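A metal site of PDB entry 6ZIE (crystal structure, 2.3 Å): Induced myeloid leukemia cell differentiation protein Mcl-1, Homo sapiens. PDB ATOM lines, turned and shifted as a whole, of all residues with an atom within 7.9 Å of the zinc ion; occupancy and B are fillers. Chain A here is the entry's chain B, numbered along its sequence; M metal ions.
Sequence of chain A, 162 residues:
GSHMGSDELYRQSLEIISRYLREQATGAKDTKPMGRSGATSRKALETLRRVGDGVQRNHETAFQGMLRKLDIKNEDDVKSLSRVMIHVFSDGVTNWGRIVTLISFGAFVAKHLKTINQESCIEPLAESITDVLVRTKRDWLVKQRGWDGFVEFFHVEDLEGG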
ATOM      1  N   LEU A  67      10.725   0.501   8.376  1.00  0.00           N
ATOM      2  CA  LEU A  67      11.743   0.038   7.438  1.00  0.00           C
ATOM      3  C   LEU A  67      13.136   0.085   8.042  1.00  0.00           C
ATOM      4  O   LEU A  67      13.904  -0.869   7.893  1.00  0.00           O
ATOM      5  CB  LEU A  67      11.670   0.872   6.153  1.00  0.00           C
ATOM      6  CG  LEU A  67      12.724   0.584   5.087  1.00  0.00           C
ATOM      7  CD1 LEU A  67      12.651  -0.867   4.608  1.00  0.00           C
ATOM      8  CD2 LEU A  67      12.566   1.516   3.915  1.00  0.00           C
ATOM      9  N   ARG A  68      13.444   1.137   8.808  1.00  0.00           N
ATOM     10  CA  ARG A  68      14.739   1.264   9.471  1.00  0.00           C
ATOM     11  C   ARG A  68      14.991   0.173  10.516  1.00  0.00           C
ATOM     12  O   ARG A  68      16.137  -0.207  10.740  1.00  0.00           O
ATOM     13  CB  ARG A  68      14.913   2.664  10.070  1.00  0.00           C
ATOM     14  CG  ARG A  68      15.031   3.776   9.028  1.00  0.00           C
ATOM     15  CD  ARG A  68      16.247   3.608   8.121  1.00  0.00           C
ATOM     16  NE  ARG A  68      17.485   3.553   8.884  1.00  0.00           N
ATOM     17  CZ  ARG A  68      18.690   3.306   8.369  1.00  0.00           C
ATOM     18  NH1 ARG A  68      18.813   3.077   7.059  1.00  0.00           N
ATOM     19  NH2 ARG A  68      19.768   3.268   9.134  1.00  0.00           N
ATOM     20  N   LEU A  70      13.987  -2.903  10.095  1.00  0.00           N
ATOM     21  CA  LEU A  70      14.206  -4.129   9.328  1.00  0.00           C
ATOM     22  C   LEU A  70      15.629  -4.142   8.754  1.00  0.00           C
ATOM     23  O   LEU A  70      16.256  -5.188   8.692  1.00  0.00           O
ATOM     24  CB  LEU A  70      13.183  -4.261   8.185  1.00  0.00           C
ATOM     25  CG  LEU A  70      11.695  -4.128   8.553  1.00  0.00           C
ATOM     26  CD1 LEU A  70      10.820  -4.404   7.350  1.00  0.00           C
ATOM     27  CD2 LEU A  70      11.302  -5.075   9.685  1.00  0.00           C
ATOM     28  N   ASP A  71      16.125  -2.967   8.317  1.00  0.00           N
ATOM     29  CA  ASP A  71      17.463  -2.836   7.754  1.00  0.00           C
ATOM     30  C   ASP A  71      18.523  -3.102   8.801  1.00  0.00           C
ATOM     31  O   ASP A  71      19.558  -3.689   8.458  1.00  0.00           O
ATOM     32  CB  ASP A  71      17.680  -1.425   7.208  1.00  0.00           C
ATOM     33  CG  ASP A  71      17.052  -1.157   5.866  1.00  0.00           C
ATOM     34  OD1 ASP A  71      16.758  -2.132   5.147  1.00  0.00           O
ATOM     35  OD2 ASP A  71      16.877   0.031   5.521  1.00  0.00           O
ATOM     36  N   ILE A  72      18.298  -2.669  10.071  1.00  0.00           N
ATOM     37  CA  ILE A  72      19.223  -2.833  11.193  1.00  0.00           C
ATOM     38  C   ILE A  72      19.783  -4.272  11.279  1.00  0.00           C
ATOM     39  O   ILE A  72      20.943  -4.457  11.657  1.00  0.00           O
ATOM     40  CB  ILE A  72      18.621  -2.340  12.529  1.00  0.00           C
ATOM     41  CG1 ILE A  72      19.726  -1.946  13.533  1.00  0.00           C
ATOM     42  CG2 ILE A  72      17.653  -3.360  13.129  1.00  0.00           C
ATOM     43  CD1 ILE A  72      19.243  -1.318  14.798  1.00  0.00           C
ATOM     44  N   LYS A  73      19.000  -5.276  10.860  1.00  0.00           N
ATOM     45  CA  LYS A  73      19.452  -6.654  10.786  1.00  0.00           C
ATOM     46  C   LYS A  73      19.729  -6.890   9.312  1.00  0.00           C
ATOM     47  O   LYS A  73      18.792  -6.862   8.513  1.00  0.00           O
ATOM     48  CB  LYS A  73      18.429  -7.641  11.384  1.00  0.00           C
ATOM     49  CG  LYS A  73      16.966  -7.450  10.945  1.00  0.00           C
ATOM     50  CD  LYS A  73      16.009  -8.282  11.784  1.00  0.00           C
ATOM     51  CE  LYS A  73      15.808  -7.658  13.142  1.00  0.00           C
ATOM     52  NZ  LYS A  73      15.220  -8.624  14.102  1.00  0.00           N
ATOM     53  N   GLU A  75      19.794  -8.187   6.165  1.00  0.00           N
ATOM     54  CA  GLU A  75      19.043  -9.299   5.580  1.00  0.00           C
ATOM     55  C   GLU A  75      18.205  -8.788   4.402  1.00  0.00           C
ATOM     56  O   GLU A  75      17.988  -7.586   4.257  1.00  0.00           O
ATOM     57  CB  GLU A  75      18.098  -9.832   6.686  1.00  0.00           C
ATOM     58  CG  GLU A  75      17.378 -11.131   6.373  1.00  0.00           C
ATOM     59  CD  GLU A  75      16.342 -11.554   7.397  1.00  0.00           C
ATOM     60  OE1 GLU A  75      16.093 -10.795   8.360  1.00  0.00           O
ATOM     61  OE2 GLU A  75      15.760 -12.652   7.221  1.00  0.00           O
ATOM     62  N   ASP A  76      17.676  -9.719   3.580  1.00  0.00           N
ATOM     63  CA  ASP A  76      16.782  -9.386   2.471  1.00  0.00           C
ATOM     64  C   ASP A  76      15.506  -8.861   3.113  1.00  0.00           C
ATOM     65  O   ASP A  76      14.858  -9.577   3.871  1.00  0.00           O
ATOM     66  CB  ASP A  76      16.528 -10.643   1.619  1.00  0.00           C
ATOM     67  CG  ASP A  76      15.770 -10.416   0.322  1.00  0.00           C
ATOM     68  OD1 ASP A  76      15.001  -9.434   0.242  1.00  0.00           O
ATOM     69  OD2 ASP A  76      15.936 -11.236  -0.599  1.00  0.00           O
ATOM     70  N   ASP A  77      15.237  -7.564   2.905  1.00  0.00           N
ATOM     71  CA  ASP A  77      14.114  -6.830   3.470  1.00  0.00           C
ATOM     72  C   ASP A  77      12.759  -7.498   3.274  1.00  0.00           C
ATOM     73  O   ASP A  77      11.876  -7.351   4.118  1.00  0.00           O
ATOM     74  CB  ASP A  77      14.090  -5.400   2.929  1.00  0.00           C
ATOM     75  CG  ASP A  77      15.283  -4.548   3.323  1.00  0.00           C
ATOM     76  OD1 ASP A  77      16.247  -5.098   3.913  1.00  0.00           O
ATOM     77  OD2 ASP A  77      15.254  -3.335   3.058  1.00  0.00           O
ATOM     78  N   VAL A  78      12.587  -8.242   2.176  1.00  0.00           N
ATOM     79  CA  VAL A  78      11.351  -8.938   1.848  1.00  0.00           C
ATOM     80  C   VAL A  78      11.111 -10.107   2.797  1.00  0.00           C
ATOM     81  O   VAL A  78       9.982 -10.332   3.240  1.00  0.00           O
ATOM     82  CB  VAL A  78      11.408  -9.419   0.385  1.00  0.00           C
ATOM     83  CG1 VAL A  78      10.142 -10.169   0.018  1.00  0.00           C
ATOM     84  CG2 VAL A  78      11.640  -8.233  -0.547  1.00  0.00           C
ATOM     85  N   VAL A 109       8.228  -0.208   0.498  1.00  0.00           N
ATOM     86  CA  VAL A 109       9.396  -1.075   0.560  1.00  0.00           C
ATOM     87  C   VAL A 109       9.965  -1.319  -0.843  1.00  0.00           C
ATOM     88  O   VAL A 109      11.178  -1.279  -1.019  1.00  0.00           O
ATOM     89  CB  VAL A 109       9.070  -2.399   1.322  1.00  0.00           C
ATOM     90  CG1 VAL A 109      10.167  -3.448   1.131  1.00  0.00           C
ATOM     91  CG2 VAL A 109       8.826  -2.146   2.796  1.00  0.00           C
ATOM     92  N   HIS A 112      12.249   1.445  -1.837  1.00  0.00           N
ATOM     93  CA  HIS A 112      13.529   1.280  -1.141  1.00  0.00           C
ATOM     94  C   HIS A 112      14.367   0.212  -1.840  1.00  0.00           C
ATOM     95  O   HIS A 112      15.565   0.392  -2.021  1.00  0.00           O
ATOM     96  CB  HIS A 112      13.274   0.938   0.341  1.00  0.00           C
ATOM     97  CG  HIS A 112      14.477   0.425   1.071  1.00  0.00           C
ATOM     98  ND1 HIS A 112      15.516   1.268   1.423  1.00  0.00           N
ATOM     99  CD2 HIS A 112      14.771  -0.829   1.488  1.00  0.00           C
ATOM    100  CE1 HIS A 112      16.399   0.507   2.043  1.00  0.00           C
ATOM    101  NE2 HIS A 112      15.992  -0.771   2.112  1.00  0.00           N
ATOM    102  N   LEU A 113      13.718  -0.887  -2.276  1.00  0.00           N
ATOM    103  CA  LEU A 113      14.372  -1.962  -3.031  1.00  0.00           C
ATOM    104  C   LEU A 113      14.907  -1.418  -4.361  1.00  0.00           C
ATOM    105  O   LEU A 113      15.970  -1.813  -4.791  1.00  0.00           O
ATOM    106  CB  LEU A 113      13.403  -3.121  -3.285  1.00  0.00           C
ATOM    107  CG  LEU A 113      13.001  -3.945  -2.055  1.00  0.00           C
ATOM    108  CD1 LEU A 113      11.919  -4.958  -2.410  1.00  0.00           C
ATOM    109  CD2 LEU A 113      14.202  -4.639  -1.439  1.00  0.00           C
ATOM    110  N   ILE A 116      18.180   0.779  -3.537  1.00  0.00           N
ATOM    111  CA  ILE A 116      19.379  -0.013  -3.240  1.00  0.00           C
ATOM    112  C   ILE A 116      19.741  -1.049  -4.325  1.00  0.00           C
ATOM    113  O   ILE A 116      20.568  -1.922  -4.069  1.00  0.00           O
ATOM    114  CB  ILE A 116      19.235  -0.689  -1.851  1.00  0.00           C
ATOM    115  CG1 ILE A 116      18.203  -1.836  -1.865  1.00  0.00           C
ATOM    116  CG2 ILE A 116      18.895   0.357  -0.770  1.00  0.00           C
ATOM    117  CD1 ILE A 116      18.168  -2.646  -0.569  1.00  0.00           C
ATOM    118  N   GLN A 118      17.851  -3.576  -5.748  1.00  0.00           N
ATOM    119  CA  GLN A 118      17.369  -4.903  -5.400  1.00  0.00           C
ATOM    120  C   GLN A 118      15.936  -5.099  -5.932  1.00  0.00           C
ATOM    121  O   GLN A 118      15.101  -5.681  -5.244  1.00  0.00           O
ATOM    122  CB  GLN A 118      17.414  -5.108  -3.870  1.00  0.00           C
ATOM    123  CG  GLN A 118      17.539  -6.557  -3.448  1.00  0.00           C
ATOM    124  CD  GLN A 118      17.438  -6.677  -1.950  1.00  0.00           C
ATOM    125  OE1 GLN A 118      18.047  -5.915  -1.206  1.00  0.00           O
ATOM    126  NE2 GLN A 118      16.663  -7.657  -1.488  1.00  0.00           N
HETATM  127 ZN    ZN M   1      16.802  -2.252   3.129  1.00  0.00          ZN
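OD2 of Asp 71 lies within salt-bridge range of NH1 of Arg 68, 3.9 Å away.
Residues that only touch the zinc ion: Ile 116. Within 4 Å of the zinc ion: Asp 71, Asp 77, His 112 and Ile 116. The nearest printed residue that does not touch the zinc ion is Leu 67 (4.6 Å).
The zinc ion is bound by the side-chain carboxylate (OD2) of Asp 77 (1.9 Å), a ring nitrogen (NE2) of His 112 (2.0 Å) and the side-chain carboxylate (OD1) of Asp 71 (2.0 Å).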
